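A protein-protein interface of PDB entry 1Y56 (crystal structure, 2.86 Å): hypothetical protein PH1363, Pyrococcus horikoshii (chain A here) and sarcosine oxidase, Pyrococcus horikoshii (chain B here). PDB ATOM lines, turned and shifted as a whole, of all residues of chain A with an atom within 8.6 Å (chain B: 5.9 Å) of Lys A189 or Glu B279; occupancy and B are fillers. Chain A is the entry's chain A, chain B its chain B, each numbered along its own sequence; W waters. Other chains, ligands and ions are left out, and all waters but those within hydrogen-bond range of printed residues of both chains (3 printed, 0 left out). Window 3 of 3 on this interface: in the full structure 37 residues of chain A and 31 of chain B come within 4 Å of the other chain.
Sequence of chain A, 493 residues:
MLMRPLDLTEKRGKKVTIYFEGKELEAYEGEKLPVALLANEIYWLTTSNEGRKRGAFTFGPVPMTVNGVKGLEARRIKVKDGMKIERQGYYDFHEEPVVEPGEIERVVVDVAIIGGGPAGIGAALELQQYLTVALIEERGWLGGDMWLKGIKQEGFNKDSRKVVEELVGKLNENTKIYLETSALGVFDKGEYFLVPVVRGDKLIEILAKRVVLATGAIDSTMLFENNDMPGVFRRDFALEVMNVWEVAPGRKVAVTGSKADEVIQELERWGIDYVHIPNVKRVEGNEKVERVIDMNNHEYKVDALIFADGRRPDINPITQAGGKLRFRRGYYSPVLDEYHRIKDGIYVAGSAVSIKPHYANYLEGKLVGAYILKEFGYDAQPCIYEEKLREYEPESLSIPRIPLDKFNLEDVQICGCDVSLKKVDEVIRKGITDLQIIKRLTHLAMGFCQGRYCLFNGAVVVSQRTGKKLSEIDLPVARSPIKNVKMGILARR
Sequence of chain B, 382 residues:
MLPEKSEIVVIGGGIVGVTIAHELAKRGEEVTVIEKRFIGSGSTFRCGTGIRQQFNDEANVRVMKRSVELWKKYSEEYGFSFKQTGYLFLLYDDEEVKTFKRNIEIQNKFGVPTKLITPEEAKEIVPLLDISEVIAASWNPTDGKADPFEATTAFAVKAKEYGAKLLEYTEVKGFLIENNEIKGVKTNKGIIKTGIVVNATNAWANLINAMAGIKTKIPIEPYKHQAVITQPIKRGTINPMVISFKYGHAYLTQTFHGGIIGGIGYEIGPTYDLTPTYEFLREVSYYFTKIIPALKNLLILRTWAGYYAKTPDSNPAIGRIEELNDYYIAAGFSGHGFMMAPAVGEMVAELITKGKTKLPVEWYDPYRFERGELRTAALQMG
Water W2 bridges O of Thr B277 and OG of Ser A480.
Water W3 lies within hydrogen-bond range of NH2 of Arg B282 (2.7 Å) and O of Leu A490 (2.8 Å).
Water W1 lies within hydrogen-bond range of the backbone NH of Tyr B278 (2.7 Å), the side-chain amino group of Lys A189 (3.1 Å) and the side-chain carboxylate of Glu B279 (3.2 Å).
The side-chain hydroxyl of Tyr B278 lies close to the guanidinium group of Arg B282 (3.5 Å).
The guanidinium group (NH1) of Arg A106 is in salt-bridge range of the side-chain carboxylate (OE2) of Glu A205.
The backbone carbonyl oxygen (O) of Phe A187 lies within hydrogen-bond range of the backbone NH (N) of Leu A194, 2.8 Å away.
Among the printed residues, merely in contact across the chains: Leu A194 with Tyr B278 (3.3 Å), Phe A187 with Tyr B278 (3.5 Å), Pro A196 with Tyr B278 (3.6 Å), Leu A490 with Leu B281 (3.6 Å), Ser A480 with Leu B281 (3.8 Å) and Arg A492 with Glu B283 (3.99 Å).
Of the 9 printed residues of chain B, 5 touch a printed residue of chain A.
Hydrophobic or aromatic side chains of chain B within 4 Å of the printed part of chain A: Tyr B278 and Leu B281.
Of the 20 printed residues of chain A, 8 touch a printed residue of chain B.
Hydrophobic or aromatic side chains of chain A that line the printed part of chain B: Phe A187, Leu A194, Pro A196 and Leu A490.
Among the printed residues, 11 pairs touch across the chains.
Among the printed residues, Asp or Glu carboxylates within 4 Å of a Lys or Arg side-chain nitrogen of the other chain: Lys A189 with Glu B279 and Glu A205 with Arg B282.
The side-chain carboxylate (OE1) of Glu A205 sits at hydrogen-bond distance from the side-chain hydroxyl (OH) of Tyr B278 (2.6 Å).
OE1 of Glu A205 is in salt-bridge range of NH1 of Arg B282, at 3.7 Å.
NZ of Lys A189 lies within salt-bridge range of OE1 of Glu B279, 2.9 Å away.
NH2 of Arg B282 lies close to O of Arg A492 (3.4 Å).
The guanidinium group of Arg B282 lies within hydrogen-bond range of the backbone carbonyl oxygen of Leu A490.
Of the printed residues of chain A, Arg B282 touches Glu A205 (3.7 Å), Leu A490 (2.8 Å) and Arg A492 (2.8 Å).
Of the printed residues of chain B, Ser A480 touches Leu B281 (3.8 Å).
Lys A343 touches none of the printed residues of chain B.
Leu A207 touches none of the printed residues of chain B.
The nearest residue of chain A that does not touch Glu B279 is Leu A194 (4.9 Å).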
ATOM      1  N   ARG A 106      29.068 -25.282  21.490  1.00  0.00           N
ATOM      2  CA  ARG A 106      28.339 -24.114  21.014  1.00  0.00           C
ATOM      3  C   ARG A 106      28.901 -22.863  21.664  1.00  0.00           C
ATOM      4  O   ARG A 106      28.901 -22.760  22.886  1.00  0.00           O
ATOM      5  CB  ARG A 106      26.859 -24.229  21.363  1.00  0.00           C
ATOM      6  CG  ARG A 106      26.018 -24.909  20.321  1.00  0.00           C
ATOM      7  CD  ARG A 106      24.871 -25.654  20.970  1.00  0.00           C
ATOM      8  NE  ARG A 106      23.628 -25.546  20.193  1.00  0.00           N
ATOM      9  CZ  ARG A 106      23.262 -26.341  19.177  1.00  0.00           C
ATOM     10  NH1 ARG A 106      24.050 -27.344  18.760  1.00  0.00           N
ATOM     11  NH2 ARG A 106      22.091 -26.123  18.571  1.00  0.00           N
ATOM     12  N   VAL A 186      28.725 -19.869   5.989  1.00  0.00           N
ATOM     13  CA  VAL A 186      27.919 -18.961   6.796  1.00  0.00           C
ATOM     14  C   VAL A 186      26.451 -19.224   6.511  1.00  0.00           C
ATOM     15  O   VAL A 186      26.043 -19.341   5.352  1.00  0.00           O
ATOM     16  CB  VAL A 186      28.253 -17.513   6.463  1.00  0.00           C
ATOM     17  CG1 VAL A 186      27.217 -16.559   7.054  1.00  0.00           C
ATOM     18  CG2 VAL A 186      29.654 -17.184   6.933  1.00  0.00           C
ATOM     19  N   PHE A 187      25.657 -19.325   7.574  1.00  0.00           N
ATOM     20  CA  PHE A 187      24.249 -19.692   7.453  1.00  0.00           C
ATOM     21  C   PHE A 187      23.395 -18.758   8.269  1.00  0.00           C
ATOM     22  O   PHE A 187      23.486 -18.743   9.491  1.00  0.00           O
ATOM     23  CB  PHE A 187      24.039 -21.113   7.927  1.00  0.00           C
ATOM     24  CG  PHE A 187      24.878 -22.110   7.213  1.00  0.00           C
ATOM     25  CD1 PHE A 187      26.119 -22.500   7.734  1.00  0.00           C
ATOM     26  CD2 PHE A 187      24.441 -22.673   6.016  1.00  0.00           C
ATOM     27  CE1 PHE A 187      26.908 -23.442   7.062  1.00  0.00           C
ATOM     28  CE2 PHE A 187      25.221 -23.622   5.346  1.00  0.00           C
ATOM     29  CZ  PHE A 187      26.456 -24.008   5.866  1.00  0.00           C
ATOM     30  N   ASP A 188      22.574 -17.978   7.570  1.00  0.00           N
ATOM     31  CA  ASP A 188      21.786 -16.917   8.169  1.00  0.00           C
ATOM     32  C   ASP A 188      20.546 -17.502   8.791  1.00  0.00           C
ATOM     33  O   ASP A 188      19.702 -18.056   8.092  1.00  0.00           O
ATOM     34  CB  ASP A 188      21.373 -15.894   7.118  1.00  0.00           C
ATOM     35  CG  ASP A 188      20.903 -14.584   7.730  1.00  0.00           C
ATOM     36  OD1 ASP A 188      20.578 -14.544   8.944  1.00  0.00           O
ATOM     37  OD2 ASP A 188      20.879 -13.572   6.994  1.00  0.00           O
ATOM     38  N   LYS A 189      20.432 -17.369  10.106  1.00  0.00           N
ATOM     39  CA  LYS A 189      19.242 -17.808  10.812  1.00  0.00           C
ATOM     40  C   LYS A 189      18.384 -16.608  11.214  1.00  0.00           C
ATOM     41  O   LYS A 189      17.589 -16.695  12.141  1.00  0.00           O
ATOM     42  CB  LYS A 189      19.634 -18.643  12.033  1.00  0.00           C
ATOM     43  CG  LYS A 189      20.584 -19.818  11.725  1.00  0.00           C
ATOM     44  CD  LYS A 189      20.008 -20.805  10.702  1.00  0.00           C
ATOM     45  CE  LYS A 189      20.430 -22.235  11.048  1.00  0.00           C
ATOM     46  NZ  LYS A 189      20.080 -23.253  10.003  1.00  0.00           N
ATOM     47  N   GLY A 190      18.543 -15.487  10.513  1.00  0.00           N
ATOM     48  CA  GLY A 190      17.771 -14.278  10.801  1.00  0.00           C
ATOM     49  C   GLY A 190      18.171 -13.583  12.088  1.00  0.00           C
ATOM     50  O   GLY A 190      18.663 -12.464  12.072  1.00  0.00           O
ATOM     51  N   GLU A 191      17.953 -14.258  13.206  1.00  0.00           N
ATOM     52  CA  GLU A 191      18.257 -13.715  14.524  1.00  0.00           C
ATOM     53  C   GLU A 191      19.741 -13.781  14.856  1.00  0.00           C
ATOM     54  O   GLU A 191      20.192 -13.111  15.779  1.00  0.00           O
ATOM     55  CB  GLU A 191      17.459 -14.468  15.590  1.00  0.00           C
ATOM     56  CG  GLU A 191      16.010 -14.028  15.714  1.00  0.00           C
ATOM     57  CD  GLU A 191      15.840 -12.764  16.545  1.00  0.00           C
ATOM     58  OE1 GLU A 191      14.874 -12.019  16.296  1.00  0.00           O
ATOM     59  OE2 GLU A 191      16.655 -12.511  17.456  1.00  0.00           O
ATOM     60  N   TYR A 192      20.480 -14.612  14.123  1.00  0.00           N
ATOM     61  CA  TYR A 192      21.939 -14.724  14.231  1.00  0.00           C
ATOM     62  C   TYR A 192      22.495 -15.451  12.988  1.00  0.00           C
ATOM     63  O   TYR A 192      21.729 -15.971  12.171  1.00  0.00           O
ATOM     64  CB  TYR A 192      22.334 -15.475  15.513  1.00  0.00           C
ATOM     65  CG  TYR A 192      21.836 -16.895  15.532  1.00  0.00           C
ATOM     66  CD1 TYR A 192      20.552 -17.204  16.002  1.00  0.00           C
ATOM     67  CD2 TYR A 192      22.630 -17.932  15.068  1.00  0.00           C
ATOM     68  CE1 TYR A 192      20.077 -18.525  15.996  1.00  0.00           C
ATOM     69  CE2 TYR A 192      22.167 -19.236  15.055  1.00  0.00           C
ATOM     70  CZ  TYR A 192      20.899 -19.526  15.522  1.00  0.00           C
ATOM     71  OH  TYR A 192      20.472 -20.826  15.513  1.00  0.00           O
ATOM     72  N   PHE A 193      23.818 -15.486  12.846  1.00  0.00           N
ATOM     73  CA  PHE A 193      24.446 -16.302  11.820  1.00  0.00           C
ATOM     74  C   PHE A 193      25.133 -17.491  12.448  1.00  0.00           C
ATOM     75  O   PHE A 193      25.776 -17.380  13.503  1.00  0.00           O
ATOM     76  CB  PHE A 193      25.487 -15.506  11.058  1.00  0.00           C
ATOM     77  CG  PHE A 193      24.934 -14.336  10.320  1.00  0.00           C
ATOM     78  CD1 PHE A 193      24.484 -14.476   9.015  1.00  0.00           C
ATOM     79  CD2 PHE A 193      24.871 -13.087  10.924  1.00  0.00           C
ATOM     80  CE1 PHE A 193      23.983 -13.401   8.328  1.00  0.00           C
ATOM     81  CE2 PHE A 193      24.361 -12.001  10.244  1.00  0.00           C
ATOM     82  CZ  PHE A 193      23.920 -12.153   8.945  1.00  0.00           C
ATOM     83  N   LEU A 194      24.994 -18.632  11.789  1.00  0.00           N
ATOM     84  CA  LEU A 194      25.736 -19.814  12.163  1.00  0.00           C
ATOM     85  C   LEU A 194      27.017 -19.996  11.320  1.00  0.00           C
ATOM     86  O   LEU A 194      26.963 -20.142  10.099  1.00  0.00           O
ATOM     87  CB  LEU A 194      24.844 -21.034  12.058  1.00  0.00           C
ATOM     88  CG  LEU A 194      25.559 -22.358  12.309  1.00  0.00           C
ATOM     89  CD1 LEU A 194      26.071 -22.438  13.742  1.00  0.00           C
ATOM     90  CD2 LEU A 194      24.601 -23.479  12.023  1.00  0.00           C
ATOM     91  N   VAL A 195      28.168 -19.962  11.973  1.00  0.00           N
ATOM     92  CA  VAL A 195      29.411 -20.262  11.299  1.00  0.00           C
ATOM     93  C   VAL A 195      29.947 -21.527  11.922  1.00  0.00           C
ATOM     94  O   VAL A 195      30.619 -21.469  12.954  1.00  0.00           O
ATOM     95  CB  VAL A 195      30.459 -19.150  11.467  1.00  0.00           C
ATOM     96  CG1 VAL A 195      31.694 -19.451  10.608  1.00  0.00           C
ATOM     97  CG2 VAL A 195      29.866 -17.793  11.115  1.00  0.00           C
ATOM     98  N   PRO A 196      29.629 -22.681  11.323  1.00  0.00           N
ATOM     99  CA  PRO A 196      30.217 -23.927  11.796  1.00  0.00           C
ATOM    100  C   PRO A 196      31.697 -23.990  11.453  1.00  0.00           C
ATOM    101  O   PRO A 196      32.121 -23.594  10.373  1.00  0.00           O
ATOM    102  CB  PRO A 196      29.441 -25.001  11.046  1.00  0.00           C
ATOM    103  CG  PRO A 196      28.851 -24.323   9.872  1.00  0.00           C
ATOM    104  CD  PRO A 196      28.712 -22.872  10.189  1.00  0.00           C
ATOM    105  N   GLU A 205      30.299 -24.869  16.695  1.00  0.00           N
ATOM    106  CA  GLU A 205      29.291 -23.992  16.106  1.00  0.00           C
ATOM    107  C   GLU A 205      29.374 -22.598  16.697  1.00  0.00           C
ATOM    108  O   GLU A 205      29.162 -22.401  17.899  1.00  0.00           O
ATOM    109  CB  GLU A 205      27.905 -24.545  16.344  1.00  0.00           C
ATOM    110  CG  GLU A 205      27.593 -25.753  15.533  1.00  0.00           C
ATOM    111  CD  GLU A 205      26.237 -26.325  15.862  1.00  0.00           C
ATOM    112  OE1 GLU A 205      25.856 -27.333  15.227  1.00  0.00           O
ATOM    113  OE2 GLU A 205      25.553 -25.770  16.752  1.00  0.00           O
ATOM    114  N   ILE A 206      29.676 -21.625  15.854  1.00  0.00           N
ATOM    115  CA  ILE A 206      29.747 -20.263  16.333  1.00  0.00           C
ATOM    116  C   ILE A 206      28.501 -19.511  15.896  1.00  0.00           C
ATOM    117  O   ILE A 206      28.219 -19.383  14.700  1.00  0.00           O
ATOM    118  CB  ILE A 206      31.033 -19.565  15.875  1.00  0.00           C
ATOM    119  CG1 ILE A 206      32.246 -20.328  16.408  1.00  0.00           C
ATOM    120  CG2 ILE A 206      31.047 -18.123  16.366  1.00  0.00           C
ATOM    121  CD1 ILE A 206      33.523 -20.089  15.653  1.00  0.00           C
ATOM    122  N   LEU A 207      27.744 -19.046  16.885  1.00  0.00           N
ATOM    123  CA  LEU A 207      26.542 -18.266  16.651  1.00  0.00           C
ATOM    124  C   LEU A 207      26.942 -16.826  16.891  1.00  0.00           C
ATOM    125  O   LEU A 207      27.359 -16.475  17.989  1.00  0.00           O
ATOM    126  CB  LEU A 207      25.415 -18.677  17.614  1.00  0.00           C
ATOM    127  CG  LEU A 207      25.010 -20.142  17.902  1.00  0.00           C
ATOM    128  CD1 LEU A 207      24.528 -20.891  16.677  1.00  0.00           C
ATOM    129  CD2 LEU A 207      26.138 -20.940  18.571  1.00  0.00           C
ATOM    130  N   ALA A 208      26.843 -15.998  15.857  1.00  0.00           N
ATOM    131  CA  ALA A 208      27.235 -14.596  15.970  1.00  0.00           C
ATOM    132  C   ALA A 208      26.185 -13.645  15.398  1.00  0.00           C
ATOM    133  O   ALA A 208      25.443 -14.014  14.484  1.00  0.00           O
ATOM    134  CB  ALA A 208      28.576 -14.372  15.302  1.00  0.00           C
ATOM    135  N   LYS A 343      25.637  -8.201   2.095  1.00  0.00           N
ATOM    136  CA  LYS A 343      24.287  -8.604   2.445  1.00  0.00           C
ATOM    137  C   LYS A 343      24.145  -8.048   3.864  1.00  0.00           C
ATOM    138  O   LYS A 343      25.155  -7.801   4.537  1.00  0.00           O
ATOM    139  CB  LYS A 343      24.210 -10.136   2.461  1.00  0.00           C
ATOM    140  CG  LYS A 343      22.849 -10.741   2.753  1.00  0.00           C
ATOM    141  CD  LYS A 343      22.950 -11.787   3.859  1.00  0.00           C
ATOM    142  CE  LYS A 343      22.983 -13.205   3.328  1.00  0.00           C
ATOM    143  NZ  LYS A 343      21.710 -13.916   3.611  1.00  0.00           N
ATOM    144  N   SER A 480      27.839 -25.711  -0.352  1.00  0.00           N
ATOM    145  CA  SER A 480      27.672 -25.901   1.094  1.00  0.00           C
ATOM    146  C   SER A 480      28.890 -25.772   1.946  1.00  0.00           C
ATOM    147  O   SER A 480      29.018 -24.730   2.590  1.00  0.00           O
ATOM    148  CB  SER A 480      26.929 -27.175   1.491  1.00  0.00           C
ATOM    149  OG  SER A 480      26.779 -27.200   2.924  1.00  0.00           O
ATOM    150  N   LEU A 490      30.931 -34.641  11.217  1.00  0.00           N
ATOM    151  CA  LEU A 490      29.610 -34.035  11.167  1.00  0.00           C
ATOM    152  C   LEU A 490      28.435 -34.895  11.680  1.00  0.00           C
ATOM    153  O   LEU A 490      27.282 -34.519  11.478  1.00  0.00           O
ATOM    154  CB  LEU A 490      29.334 -33.559   9.748  1.00  0.00           C
ATOM    155  CG  LEU A 490      29.660 -32.152   9.245  1.00  0.00           C
ATOM    156  CD1 LEU A 490      30.831 -31.530   9.935  1.00  0.00           C
ATOM    157  CD2 LEU A 490      29.907 -32.228   7.766  1.00  0.00           C
ATOM    158  N   ARG A 492      27.113 -37.059  15.533  1.00  0.00           N
ATOM    159  CA  ARG A 492      25.719 -36.620  15.501  1.00  0.00           C
ATOM    160  C   ARG A 492      25.817 -35.297  16.220  1.00  0.00           C
ATOM    161  O   ARG A 492      26.673 -35.143  17.097  1.00  0.00           O
ATOM    162  CB  ARG A 492      24.810 -37.556  16.327  1.00  0.00           C
ATOM    163  CG  ARG A 492      23.546 -36.900  16.942  1.00  0.00           C
ATOM    164  CD  ARG A 492      22.203 -37.387  16.335  1.00  0.00           C
ATOM    165  NE  ARG A 492      21.773 -36.656  15.123  1.00  0.00           N
ATOM    166  CZ  ARG A 492      20.657 -36.909  14.415  1.00  0.00           C
ATOM    167  NH1 ARG A 492      20.366 -36.190  13.329  1.00  0.00           N
ATOM    168  NH2 ARG A 492      19.819 -37.877  14.777  1.00  0.00           N
ATOM    169  N   TYR B 266      14.972 -35.569   3.922  1.00  0.00           N
ATOM    170  CA  TYR B 266      14.895 -34.151   4.324  1.00  0.00           C
ATOM    171  C   TYR B 266      14.366 -33.161   3.272  1.00  0.00           C
ATOM    172  O   TYR B 266      15.108 -32.652   2.438  1.00  0.00           O
ATOM    173  CB  TYR B 266      16.260 -33.709   4.863  1.00  0.00           C
ATOM    174  CG  TYR B 266      16.280 -32.359   5.561  1.00  0.00           C
ATOM    175  CD1 TYR B 266      15.839 -32.216   6.881  1.00  0.00           C
ATOM    176  CD2 TYR B 266      16.764 -31.232   4.905  1.00  0.00           C
ATOM    177  CE1 TYR B 266      15.866 -30.973   7.519  1.00  0.00           C
ATOM    178  CE2 TYR B 266      16.794 -29.996   5.526  1.00  0.00           C
ATOM    179  CZ  TYR B 266      16.349 -29.866   6.828  1.00  0.00           C
ATOM    180  OH  TYR B 266      16.403 -28.619   7.415  1.00  0.00           O
ATOM    181  N   THR B 277      21.619 -26.440   2.824  1.00  0.00           N
ATOM    182  CA  THR B 277      21.479 -26.035   4.214  1.00  0.00           C
ATOM    183  C   THR B 277      22.429 -26.816   5.125  1.00  0.00           C
ATOM    184  O   THR B 277      22.693 -27.989   4.892  1.00  0.00           O
ATOM    185  CB  THR B 277      20.003 -26.184   4.688  1.00  0.00           C
ATOM    186  OG1 THR B 277      19.726 -27.544   5.049  1.00  0.00           O
ATOM    187  CG2 THR B 277      19.042 -25.751   3.586  1.00  0.00           C
ATOM    188  N   TYR B 278      22.921 -26.162   6.176  1.00  0.00           N
ATOM    189  CA  TYR B 278      23.744 -26.805   7.229  1.00  0.00           C
ATOM    190  C   TYR B 278      23.105 -28.029   7.887  1.00  0.00           C
ATOM    191  O   TYR B 278      23.812 -28.980   8.240  1.00  0.00           O
ATOM    192  CB  TYR B 278      24.120 -25.793   8.317  1.00  0.00           C
ATOM    193  CG  TYR B 278      24.815 -26.386   9.525  1.00  0.00           C
ATOM    194  CD1 TYR B 278      26.137 -26.819   9.451  1.00  0.00           C
ATOM    195  CD2 TYR B 278      24.147 -26.508  10.752  1.00  0.00           C
ATOM    196  CE1 TYR B 278      26.774 -27.366  10.563  1.00  0.00           C
ATOM    197  CE2 TYR B 278      24.777 -27.043  11.871  1.00  0.00           C
ATOM    198  CZ  TYR B 278      26.091 -27.467  11.768  1.00  0.00           C
ATOM    199  OH  TYR B 278      26.725 -28.002  12.867  1.00  0.00           O
ATOM    200  N   GLU B 279      21.744 -28.081   7.881  1.00  0.00           N
ATOM    201  CA  GLU B 279      21.018 -29.039   8.696  1.00  0.00           C
ATOM    202  C   GLU B 279      21.097 -30.363   7.888  1.00  0.00           C
ATOM    203  O   GLU B 279      21.343 -31.443   8.455  1.00  0.00           O
ATOM    204  CB  GLU B 279      19.527 -28.654   8.834  1.00  0.00           C
ATOM    205  CG  GLU B 279      19.270 -27.119   8.721  1.00  0.00           C
ATOM    206  CD  GLU B 279      19.753 -26.408   9.984  1.00  0.00           C
ATOM    207  OE1 GLU B 279      20.940 -25.979  10.027  1.00  0.00           O
ATOM    208  OE2 GLU B 279      18.962 -26.311  10.970  1.00  0.00           O
ATOM    209  N   PHE B 280      20.897 -30.237   6.563  1.00  0.00           N
ATOM    210  CA  PHE B 280      21.112 -31.344   5.641  1.00  0.00           C
ATOM    211  C   PHE B 280      22.522 -31.888   5.736  1.00  0.00           C
ATOM    212  O   PHE B 280      22.701 -33.101   5.712  1.00  0.00           O
ATOM    213  CB  PHE B 280      20.822 -30.958   4.192  1.00  0.00           C
ATOM    214  CG  PHE B 280      21.321 -31.963   3.199  1.00  0.00           C
ATOM    215  CD1 PHE B 280      20.658 -33.172   3.024  1.00  0.00           C
ATOM    216  CD2 PHE B 280      22.474 -31.716   2.460  1.00  0.00           C
ATOM    217  CE1 PHE B 280      21.127 -34.120   2.118  1.00  0.00           C
ATOM    218  CE2 PHE B 280      22.953 -32.661   1.553  1.00  0.00           C
ATOM    219  CZ  PHE B 280      22.276 -33.866   1.384  1.00  0.00           C
ATOM    220  N   LEU B 281      23.511 -30.994   5.827  1.00  0.00           N
ATOM    221  CA  LEU B 281      24.920 -31.386   5.931  1.00  0.00           C
ATOM    222  C   LEU B 281      25.129 -32.314   7.126  1.00  0.00           C
ATOM    223  O   LEU B 281      25.800 -33.340   7.029  1.00  0.00           O
ATOM    224  CB  LEU B 281      25.807 -30.153   6.104  1.00  0.00           C
ATOM    225  CG  LEU B 281      27.187 -30.002   5.433  1.00  0.00           C
ATOM    226  CD1 LEU B 281      28.155 -29.335   6.403  1.00  0.00           C
ATOM    227  CD2 LEU B 281      27.776 -31.314   4.915  1.00  0.00           C
ATOM    228  N   ARG B 282      24.526 -31.942   8.250  1.00  0.00           N
ATOM    229  CA  ARG B 282      24.648 -32.699   9.482  1.00  0.00           C
ATOM    230  C   ARG B 282      23.920 -34.017   9.400  1.00  0.00           C
ATOM    231  O   ARG B 282      24.456 -35.045   9.782  1.00  0.00           O
ATOM    232  CB  ARG B 282      24.096 -31.889  10.655  1.00  0.00           C
ATOM    233  CG  ARG B 282      24.905 -30.644  10.972  1.00  0.00           C
ATOM    234  CD  ARG B 282      26.283 -30.995  11.497  1.00  0.00           C
ATOM    235  NE  ARG B 282      26.253 -32.138  12.411  1.00  0.00           N
ATOM    236  CZ  ARG B 282      25.905 -32.087  13.695  1.00  0.00           C
ATOM    237  NH1 ARG B 282      25.546 -30.942  14.262  1.00  0.00           N
ATOM    238  NH2 ARG B 282      25.916 -33.193  14.422  1.00  0.00           N
ATOM    239  N   GLU B 283      22.691 -33.977   8.906  1.00  0.00           N
ATOM    240  CA  GLU B 283      21.852 -35.165   8.853  1.00  0.00           C
ATOM    241  C   GLU B 283      22.395 -36.229   7.899  1.00  0.00           C
ATOM    242  O   GLU B 283      22.533 -37.380   8.278  1.00  0.00           O
ATOM    243  CB  GLU B 283      20.404 -34.793   8.539  1.00  0.00           C
ATOM    244  CG  GLU B 283      19.521 -34.632   9.754  1.00  0.00           C
ATOM    245  CD  GLU B 283      18.074 -34.310   9.377  1.00  0.00           C
ATOM    246  OE1 GLU B 283      17.776 -33.134   9.074  1.00  0.00           O
ATOM    247  OE2 GLU B 283      17.218 -35.224   9.381  1.00  0.00           O
ATOM    248  N   VAL B 284      22.731 -35.842   6.675  1.00  0.00           N
ATOM    249  CA  VAL B 284      23.309 -36.790   5.724  1.00  0.00           C
ATOM    250  C   VAL B 284      24.570 -37.467   6.290  1.00  0.00           C
ATOM    251  O   VAL B 284      24.760 -38.676   6.128  1.00  0.00           O
ATOM    252  CB  VAL B 284      23.594 -36.157   4.341  1.00  0.00           C
ATOM    253  CG1 VAL B 284      24.847 -35.296   4.367  1.00  0.00           C
ATOM    254  CG2 VAL B 284      23.725 -37.235   3.309  1.00  0.00           C
HETATM  255  O   HOH W   1      21.288 -24.326   7.326  1.00  0.00           O
HETATM  256  O   HOH W   2      24.509 -28.277   3.224  1.00  0.00           O
HETATM  257  O   HOH W   3      24.996 -35.217  12.868  1.00  0.00           O
